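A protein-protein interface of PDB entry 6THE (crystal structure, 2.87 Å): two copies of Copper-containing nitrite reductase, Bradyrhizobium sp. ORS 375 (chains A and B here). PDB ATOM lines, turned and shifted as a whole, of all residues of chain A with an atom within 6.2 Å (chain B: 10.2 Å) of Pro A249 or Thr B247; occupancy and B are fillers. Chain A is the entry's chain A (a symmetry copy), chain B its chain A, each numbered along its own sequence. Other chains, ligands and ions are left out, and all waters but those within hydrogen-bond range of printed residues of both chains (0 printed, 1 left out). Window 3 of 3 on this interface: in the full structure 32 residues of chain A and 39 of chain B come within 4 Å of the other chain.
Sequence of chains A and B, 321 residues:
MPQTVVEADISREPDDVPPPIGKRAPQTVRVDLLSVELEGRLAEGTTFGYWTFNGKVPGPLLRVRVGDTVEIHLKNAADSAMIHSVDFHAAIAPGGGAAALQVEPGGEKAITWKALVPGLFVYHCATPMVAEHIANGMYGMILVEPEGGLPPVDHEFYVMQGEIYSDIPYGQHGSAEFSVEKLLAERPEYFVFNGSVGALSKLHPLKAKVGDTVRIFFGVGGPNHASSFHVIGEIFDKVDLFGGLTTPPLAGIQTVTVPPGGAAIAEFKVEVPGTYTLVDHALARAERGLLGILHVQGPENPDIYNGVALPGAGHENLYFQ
N of Ala A251 lies within hydrogen-bond range of OG1 of Thr B247, at 2.9 Å.
The backbone carbonyl oxygen of Val A239 lies within hydrogen-bond range of the backbone NH of Leu A250.
Leu A241 touches Phe B242. Pro A249 touches Thr B247 (O to OG1, 3.98 Å). Thr B247 touches Leu A250. Ala A251 touches Thr B246. Val B117 touches Gly A252. Gly A252 touches Gly B244 (O to CA, 3.8 Å). Ile A253 touches Phe B242.
Of chain B, only Thr B247 (3.98 Å) comes within 4 Å of Pro A249. Of chain A, only Pro A249, Leu A250 and Ala A251 come within 4 Å of Thr B247. No residue of chain B comes within 4 Å of Pro A248. Of the printed residues of chain A, Gly B244 touches Gly A252 (3.8 Å). Of the printed residues of chain B, Leu A241 touches Phe B242 (3.8 Å). Gly B243 touches none of the printed residues of chain A. Thr A247 touches none of the printed residues of chain B. The nearest residue of chain B that does not touch Pro A249 is Pro B248 (7.3 Å). The nearest residue of chain A that does not touch Thr B247 is Ile A253 (5.6 Å). The nearest printed residue of chain A that does not touch Val B117 is Ile A253 (5.2 Å).
Of the 11 printed residues of chain A, 6 touch a printed residue of chain B.
Pro A249 touches Thr B247, but with the chains exchanged Thr A247 does not touch Pro B249 (11.3 Å). Leu A250 touches Thr B247, but with the chains exchanged Thr A247 does not touch Leu B250 (9.1 Å). Ala A251 touches Thr B247, but with the chains exchanged Thr A247 does not touch Ala B251 (12.7 Å). 9 positions are printed for both chains.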
ATOM      1  N   LYS A 238      14.016 -33.128  39.145  1.00  0.00           N
ATOM      2  CA  LYS A 238      14.184 -34.216  38.194  1.00  0.00           C
ATOM      3  C   LYS A 238      12.820 -34.806  37.845  1.00  0.00           C
ATOM      4  O   LYS A 238      11.997 -35.042  38.729  1.00  0.00           O
ATOM      5  CB  LYS A 238      15.129 -35.284  38.753  1.00  0.00           C
ATOM      6  CG  LYS A 238      16.609 -34.925  38.714  1.00  0.00           C
ATOM      7  CD  LYS A 238      17.467 -35.776  39.625  1.00  0.00           C
ATOM      8  CE  LYS A 238      18.884 -35.255  39.751  1.00  0.00           C
ATOM      9  NZ  LYS A 238      19.659 -36.010  40.763  1.00  0.00           N
ATOM     10  N   VAL A 239      12.598 -35.031  36.545  1.00  0.00           N
ATOM     11  CA  VAL A 239      11.365 -35.620  36.044  1.00  0.00           C
ATOM     12  C   VAL A 239      11.715 -36.769  35.102  1.00  0.00           C
ATOM     13  O   VAL A 239      12.435 -36.578  34.122  1.00  0.00           O
ATOM     14  CB  VAL A 239      10.467 -34.575  35.349  1.00  0.00           C
ATOM     15  CG1 VAL A 239       9.313 -35.222  34.595  1.00  0.00           C
ATOM     16  CG2 VAL A 239       9.940 -33.532  36.322  1.00  0.00           C
ATOM     17  N   ASP A 240      11.195 -37.960  35.421  1.00  0.00           N
ATOM     18  CA  ASP A 240      11.267 -39.107  34.529  1.00  0.00           C
ATOM     19  C   ASP A 240      10.053 -39.073  33.605  1.00  0.00           C
ATOM     20  O   ASP A 240       8.944 -39.412  34.015  1.00  0.00           O
ATOM     21  CB  ASP A 240      11.401 -40.416  35.311  1.00  0.00           C
ATOM     22  CG  ASP A 240      12.685 -40.511  36.119  1.00  0.00           C
ATOM     23  OD1 ASP A 240      13.770 -40.452  35.507  1.00  0.00           O
ATOM     24  OD2 ASP A 240      12.591 -40.640  37.355  1.00  0.00           O
ATOM     25  N   LEU A 241      10.287 -38.645  32.358  1.00  0.00           N
ATOM     26  CA  LEU A 241       9.233 -38.403  31.386  1.00  0.00           C
ATOM     27  C   LEU A 241       8.599 -39.728  30.970  1.00  0.00           C
ATOM     28  O   LEU A 241       9.300 -40.665  30.590  1.00  0.00           O
ATOM     29  CB  LEU A 241       9.832 -37.664  30.182  1.00  0.00           C
ATOM     30  CG  LEU A 241       8.832 -37.005  29.232  1.00  0.00           C
ATOM     31  CD1 LEU A 241       8.147 -35.816  29.893  1.00  0.00           C
ATOM     32  CD2 LEU A 241       9.516 -36.571  27.946  1.00  0.00           C
ATOM     33  N   THR A 247      16.423 -43.712  30.304  1.00  0.00           N
ATOM     34  CA  THR A 247      17.011 -42.472  29.822  1.00  0.00           C
ATOM     35  C   THR A 247      17.169 -41.508  30.997  1.00  0.00           C
ATOM     36  O   THR A 247      16.269 -41.403  31.830  1.00  0.00           O
ATOM     37  CB  THR A 247      16.175 -41.899  28.667  1.00  0.00           C
ATOM     38  OG1 THR A 247      16.253 -42.820  27.579  1.00  0.00           O
ATOM     39  CG2 THR A 247      16.631 -40.534  28.200  1.00  0.00           C
ATOM     40  N   PRO A 248      18.317 -40.794  31.114  1.00  0.00           N
ATOM     41  CA  PRO A 248      18.504 -39.778  32.154  1.00  0.00           C
ATOM     42  C   PRO A 248      17.349 -38.778  32.222  1.00  0.00           C
ATOM     43  O   PRO A 248      16.829 -38.360  31.189  1.00  0.00           O
ATOM     44  CB  PRO A 248      19.790 -39.061  31.718  1.00  0.00           C
ATOM     45  CG  PRO A 248      20.567 -40.122  30.972  1.00  0.00           C
ATOM     46  CD  PRO A 248      19.512 -40.951  30.267  1.00  0.00           C
ATOM     47  N   PRO A 249      16.922 -38.362  33.438  1.00  0.00           N
ATOM     48  CA  PRO A 249      15.738 -37.514  33.595  1.00  0.00           C
ATOM     49  C   PRO A 249      15.958 -36.063  33.173  1.00  0.00           C
ATOM     50  O   PRO A 249      17.093 -35.595  33.094  1.00  0.00           O
ATOM     51  CB  PRO A 249      15.463 -37.581  35.106  1.00  0.00           C
ATOM     52  CG  PRO A 249      16.825 -37.812  35.723  1.00  0.00           C
ATOM     53  CD  PRO A 249      17.559 -38.685  34.725  1.00  0.00           C
ATOM     54  N   LEU A 250      14.847 -35.368  32.900  1.00  0.00           N
ATOM     55  CA  LEU A 250      14.846 -33.939  32.624  1.00  0.00           C
ATOM     56  C   LEU A 250      15.094 -33.186  33.928  1.00  0.00           C
ATOM     57  O   LEU A 250      14.821 -33.706  35.008  1.00  0.00           O
ATOM     58  CB  LEU A 250      13.493 -33.552  32.017  1.00  0.00           C
ATOM     59  CG  LEU A 250      13.297 -33.898  30.541  1.00  0.00           C
ATOM     60  CD1 LEU A 250      11.817 -34.012  30.205  1.00  0.00           C
ATOM     61  CD2 LEU A 250      13.970 -32.869  29.644  1.00  0.00           C
ATOM     62  N   ALA A 251      15.607 -31.954  33.812  1.00  0.00           N
ATOM     63  CA  ALA A 251      15.988 -31.173  34.978  1.00  0.00           C
ATOM     64  C   ALA A 251      15.383 -29.773  34.910  1.00  0.00           C
ATOM     65  O   ALA A 251      15.488 -29.093  33.891  1.00  0.00           O
ATOM     66  CB  ALA A 251      17.492 -31.128  35.099  1.00  0.00           C
ATOM     67  N   GLY A 252      14.746 -29.366  36.016  1.00  0.00           N
ATOM     68  CA  GLY A 252      14.226 -28.020  36.193  1.00  0.00           C
ATOM     69  C   GLY A 252      12.985 -27.756  35.346  1.00  0.00           C
ATOM     70  O   GLY A 252      13.002 -26.888  34.474  1.00  0.00           O
ATOM     71  N   ILE A 253      11.912 -28.506  35.624  1.00  0.00           N
ATOM     72  CA  ILE A 253      10.676 -28.421  34.860  1.00  0.00           C
ATOM     73  C   ILE A 253       9.557 -27.904  35.764  1.00  0.00           C
ATOM     74  O   ILE A 253       9.450 -28.301  36.922  1.00  0.00           O
ATOM     75  CB  ILE A 253      10.351 -29.773  34.186  1.00  0.00           C
ATOM     76  CG1 ILE A 253      10.951 -29.864  32.779  1.00  0.00           C
ATOM     77  CG2 ILE A 253       8.853 -30.049  34.159  1.00  0.00           C
ATOM     78  CD1 ILE A 253      12.444 -30.111  32.743  1.00  0.00           C
ATOM     79  N   VAL B 117      16.416 -21.966  39.572  1.00  0.00           N
ATOM     80  CA  VAL B 117      16.336 -22.868  38.434  1.00  0.00           C
ATOM     81  C   VAL B 117      16.301 -22.046  37.145  1.00  0.00           C
ATOM     82  O   VAL B 117      15.473 -21.147  37.005  1.00  0.00           O
ATOM     83  CB  VAL B 117      15.121 -23.813  38.544  1.00  0.00           C
ATOM     84  CG1 VAL B 117      14.945 -24.669  37.298  1.00  0.00           C
ATOM     85  CG2 VAL B 117      15.192 -24.690  39.786  1.00  0.00           C
ATOM     86  N   PRO B 118      17.201 -22.326  36.172  1.00  0.00           N
ATOM     87  CA  PRO B 118      17.154 -21.670  34.864  1.00  0.00           C
ATOM     88  C   PRO B 118      16.016 -22.212  34.002  1.00  0.00           C
ATOM     89  O   PRO B 118      15.639 -23.377  34.124  1.00  0.00           O
ATOM     90  CB  PRO B 118      18.509 -22.028  34.234  1.00  0.00           C
ATOM     91  CG  PRO B 118      18.894 -23.340  34.888  1.00  0.00           C
ATOM     92  CD  PRO B 118      18.322 -23.274  36.288  1.00  0.00           C
ATOM     93  N   GLY B 119      15.479 -21.347  33.136  1.00  0.00           N
ATOM     94  CA  GLY B 119      14.423 -21.734  32.216  1.00  0.00           C
ATOM     95  C   GLY B 119      13.365 -20.647  32.050  1.00  0.00           C
ATOM     96  O   GLY B 119      13.412 -19.614  32.716  1.00  0.00           O
ATOM     97  N   PRO B 146      20.606 -18.947  32.445  1.00  0.00           N
ATOM     98  CA  PRO B 146      21.632 -19.667  33.203  1.00  0.00           C
ATOM     99  C   PRO B 146      22.917 -18.856  33.366  1.00  0.00           C
ATOM    100  O   PRO B 146      23.023 -17.744  32.853  1.00  0.00           O
ATOM    101  CB  PRO B 146      21.892 -20.917  32.347  1.00  0.00           C
ATOM    102  CG  PRO B 146      21.549 -20.482  30.939  1.00  0.00           C
ATOM    103  CD  PRO B 146      20.388 -19.523  31.107  1.00  0.00           C
ATOM    104  N   LEU B 150      22.118 -17.183  27.385  1.00  0.00           N
ATOM    105  CA  LEU B 150      21.770 -17.857  26.145  1.00  0.00           C
ATOM    106  C   LEU B 150      22.688 -17.372  25.025  1.00  0.00           C
ATOM    107  O   LEU B 150      23.078 -16.205  25.008  1.00  0.00           O
ATOM    108  CB  LEU B 150      20.305 -17.554  25.809  1.00  0.00           C
ATOM    109  CG  LEU B 150      19.259 -18.321  26.617  1.00  0.00           C
ATOM    110  CD1 LEU B 150      17.902 -17.639  26.526  1.00  0.00           C
ATOM    111  CD2 LEU B 150      19.159 -19.766  26.151  1.00  0.00           C
ATOM    112  N   LYS B 238      16.397 -26.060  17.724  1.00  0.00           N
ATOM    113  CA  LYS B 238      16.538 -26.401  19.131  1.00  0.00           C
ATOM    114  C   LYS B 238      15.255 -26.041  19.876  1.00  0.00           C
ATOM    115  O   LYS B 238      14.701 -24.960  19.680  1.00  0.00           O
ATOM    116  CB  LYS B 238      17.755 -25.695  19.739  1.00  0.00           C
ATOM    117  CG  LYS B 238      19.104 -26.305  19.381  1.00  0.00           C
ATOM    118  CD  LYS B 238      20.276 -25.381  19.631  1.00  0.00           C
ATOM    119  CE  LYS B 238      21.573 -25.910  19.054  1.00  0.00           C
ATOM    120  NZ  LYS B 238      22.671 -24.922  19.174  1.00  0.00           N
ATOM    121  N   VAL B 239      14.796 -26.968  20.725  1.00  0.00           N
ATOM    122  CA  VAL B 239      13.605 -26.774  21.539  1.00  0.00           C
ATOM    123  C   VAL B 239      13.934 -27.128  22.986  1.00  0.00           C
ATOM    124  O   VAL B 239      14.376 -28.240  23.273  1.00  0.00           O
ATOM    125  CB  VAL B 239      12.408 -27.595  21.015  1.00  0.00           C
ATOM    126  CG1 VAL B 239      11.248 -27.608  22.001  1.00  0.00           C
ATOM    127  CG2 VAL B 239      11.935 -27.116  19.652  1.00  0.00           C
ATOM    128  N   ASP B 240      13.713 -26.162  23.885  1.00  0.00           N
ATOM    129  CA  ASP B 240      13.786 -26.398  25.318  1.00  0.00           C
ATOM    130  C   ASP B 240      12.411 -26.855  25.800  1.00  0.00           C
ATOM    131  O   ASP B 240      11.496 -26.045  25.940  1.00  0.00           O
ATOM    132  CB  ASP B 240      14.315 -25.169  26.062  1.00  0.00           C
ATOM    133  CG  ASP B 240      15.741 -24.801  25.687  1.00  0.00           C
ATOM    134  OD1 ASP B 240      16.638 -25.645  25.891  1.00  0.00           O
ATOM    135  OD2 ASP B 240      15.945 -23.676  25.192  1.00  0.00           O
ATOM    136  N   LEU B 241      12.288 -28.167  26.035  1.00  0.00           N
ATOM    137  CA  LEU B 241      11.020 -28.805  26.353  1.00  0.00           C
ATOM    138  C   LEU B 241      10.551 -28.362  27.737  1.00  0.00           C
ATOM    139  O   LEU B 241      11.304 -28.440  28.707  1.00  0.00           O
ATOM    140  CB  LEU B 241      11.201 -30.326  26.281  1.00  0.00           C
ATOM    141  CG  LEU B 241       9.917 -31.155  26.223  1.00  0.00           C
ATOM    142  CD1 LEU B 241       9.198 -30.962  24.894  1.00  0.00           C
ATOM    143  CD2 LEU B 241      10.216 -32.628  26.452  1.00  0.00           C
ATOM    144  N   PHE B 242       9.296 -27.893  27.795  1.00  0.00           N
ATOM    145  CA  PHE B 242       8.660 -27.367  28.996  1.00  0.00           C
ATOM    146  C   PHE B 242       9.358 -26.088  29.457  1.00  0.00           C
ATOM    147  O   PHE B 242       9.092 -25.593  30.551  1.00  0.00           O
ATOM    148  CB  PHE B 242       8.558 -28.434  30.091  1.00  0.00           C
ATOM    149  CG  PHE B 242       7.831 -29.694  29.689  1.00  0.00           C
ATOM    150  CD1 PHE B 242       6.493 -29.659  29.323  1.00  0.00           C
ATOM    151  CD2 PHE B 242       8.483 -30.918  29.688  1.00  0.00           C
ATOM    152  CE1 PHE B 242       5.825 -30.819  28.957  1.00  0.00           C
ATOM    153  CE2 PHE B 242       7.814 -32.077  29.321  1.00  0.00           C
ATOM    154  CZ  PHE B 242       6.487 -32.026  28.957  1.00  0.00           C
ATOM    155  N   GLY B 243      10.240 -25.560  28.599  1.00  0.00           N
ATOM    156  CA  GLY B 243      10.961 -24.323  28.856  1.00  0.00           C
ATOM    157  C   GLY B 243      11.998 -24.474  29.966  1.00  0.00           C
ATOM    158  O   GLY B 243      12.139 -23.589  30.806  1.00  0.00           O
ATOM    159  N   GLY B 244      12.713 -25.605  29.958  1.00  0.00           N
ATOM    160  CA  GLY B 244      13.771 -25.865  30.921  1.00  0.00           C
ATOM    161  C   GLY B 244      15.150 -25.643  30.304  1.00  0.00           C
ATOM    162  O   GLY B 244      15.435 -26.153  29.222  1.00  0.00           O
ATOM    163  N   LEU B 245      15.992 -24.875  31.007  1.00  0.00           N
ATOM    164  CA  LEU B 245      17.322 -24.539  30.526  1.00  0.00           C
ATOM    165  C   LEU B 245      18.380 -25.200  31.407  1.00  0.00           C
ATOM    166  O   LEU B 245      19.359 -24.563  31.790  1.00  0.00           O
ATOM    167  CB  LEU B 245      17.486 -23.015  30.507  1.00  0.00           C
ATOM    168  CG  LEU B 245      16.833 -22.282  29.334  1.00  0.00           C
ATOM    169  CD1 LEU B 245      16.865 -20.777  29.554  1.00  0.00           C
ATOM    170  CD2 LEU B 245      17.509 -22.638  28.018  1.00  0.00           C
ATOM    171  N   THR B 246      18.172 -26.485  31.713  1.00  0.00           N
ATOM    172  CA  THR B 246      19.133 -27.258  32.485  1.00  0.00           C
ATOM    173  C   THR B 246      19.586 -28.463  31.664  1.00  0.00           C
ATOM    174  O   THR B 246      20.784 -28.675  31.477  1.00  0.00           O
ATOM    175  CB  THR B 246      18.571 -27.639  33.862  1.00  0.00           C
ATOM    176  OG1 THR B 246      17.829 -26.532  34.379  1.00  0.00           O
ATOM    177  CG2 THR B 246      19.649 -28.035  34.849  1.00  0.00           C
ATOM    178  N   THR B 247      18.608 -29.238  31.177  1.00  0.00           N
ATOM    179  CA  THR B 247      18.851 -30.383  30.313  1.00  0.00           C
ATOM    180  C   THR B 247      19.093 -29.886  28.888  1.00  0.00           C
ATOM    181  O   THR B 247      18.394 -28.986  28.424  1.00  0.00           O
ATOM    182  CB  THR B 247      17.694 -31.389  30.424  1.00  0.00           C
ATOM    183  OG1 THR B 247      17.691 -31.897  31.758  1.00  0.00           O
ATOM    184  CG2 THR B 247      17.791 -32.542  29.450  1.00  0.00           C
ATOM    185  N   PRO B 248      20.096 -30.438  28.160  1.00  0.00           N
ATOM    186  CA  PRO B 248      20.327 -30.088  26.755  1.00  0.00           C
ATOM    187  C   PRO B 248      19.059 -30.177  25.905  1.00  0.00           C
ATOM    188  O   PRO B 248      18.260 -31.096  26.076  1.00  0.00           O
ATOM    189  CB  PRO B 248      21.341 -31.145  26.291  1.00  0.00           C
ATOM    190  CG  PRO B 248      22.107 -31.494  27.547  1.00  0.00           C
ATOM    191  CD  PRO B 248      21.084 -31.408  28.662  1.00  0.00           C
ATOM    192  N   PRO B 249      18.843 -29.229  24.961  1.00  0.00           N
ATOM    193  CA  PRO B 249      17.594 -29.164  24.200  1.00  0.00           C
ATOM    194  C   PRO B 249      17.460 -30.254  23.139  1.00  0.00           C
ATOM    195  O   PRO B 249      18.450 -30.853  22.722  1.00  0.00           O
ATOM    196  CB  PRO B 249      17.674 -27.786  23.523  1.00  0.00           C
ATOM    197  CG  PRO B 249      19.157 -27.537  23.358  1.00  0.00           C
ATOM    198  CD  PRO B 249      19.795 -28.173  24.576  1.00  0.00           C
ATOM    199  N   LEU B 250      16.211 -30.499  22.720  1.00  0.00           N
ATOM    200  CA  LEU B 250      15.901 -31.395  21.617  1.00  0.00           C
ATOM    201  C   LEU B 250      16.294 -30.718  20.307  1.00  0.00           C
ATOM    202  O   LEU B 250      16.360 -29.492  20.236  1.00  0.00           O
ATOM    203  CB  LEU B 250      14.401 -31.711  21.641  1.00  0.00           C
ATOM    204  CG  LEU B 250      13.949 -32.737  22.681  1.00  0.00           C
ATOM    205  CD1 LEU B 250      12.475 -32.556  23.012  1.00  0.00           C
ATOM    206  CD2 LEU B 250      14.218 -34.156  22.201  1.00  0.00           C
ATOM    207  N   ALA B 251      16.547 -31.530  19.272  1.00  0.00           N
ATOM    208  CA  ALA B 251      17.033 -31.019  18.001  1.00  0.00           C
ATOM    209  C   ALA B 251      16.193 -31.559  16.846  1.00  0.00           C
ATOM    210  O   ALA B 251      15.951 -32.762  16.755  1.00  0.00           O
ATOM    211  CB  ALA B 251      18.495 -31.355  17.836  1.00  0.00           C
ATOM    212  N   ILE B 265      11.134 -22.966  24.468  1.00  0.00           N
ATOM    213  CA  ILE B 265      12.051 -22.078  23.774  1.00  0.00           C
ATOM    214  C   ILE B 265      12.381 -22.706  22.422  1.00  0.00           C
ATOM    215  O   ILE B 265      13.154 -23.660  22.343  1.00  0.00           O
ATOM    216  CB  ILE B 265      13.307 -21.785  24.622  1.00  0.00           C
ATOM    217  CG1 ILE B 265      12.949 -21.114  25.952  1.00  0.00           C
ATOM    218  CG2 ILE B 265      14.317 -20.962  23.833  1.00  0.00           C
ATOM    219  CD1 ILE B 265      14.051 -21.158  26.987  1.00  0.00           C
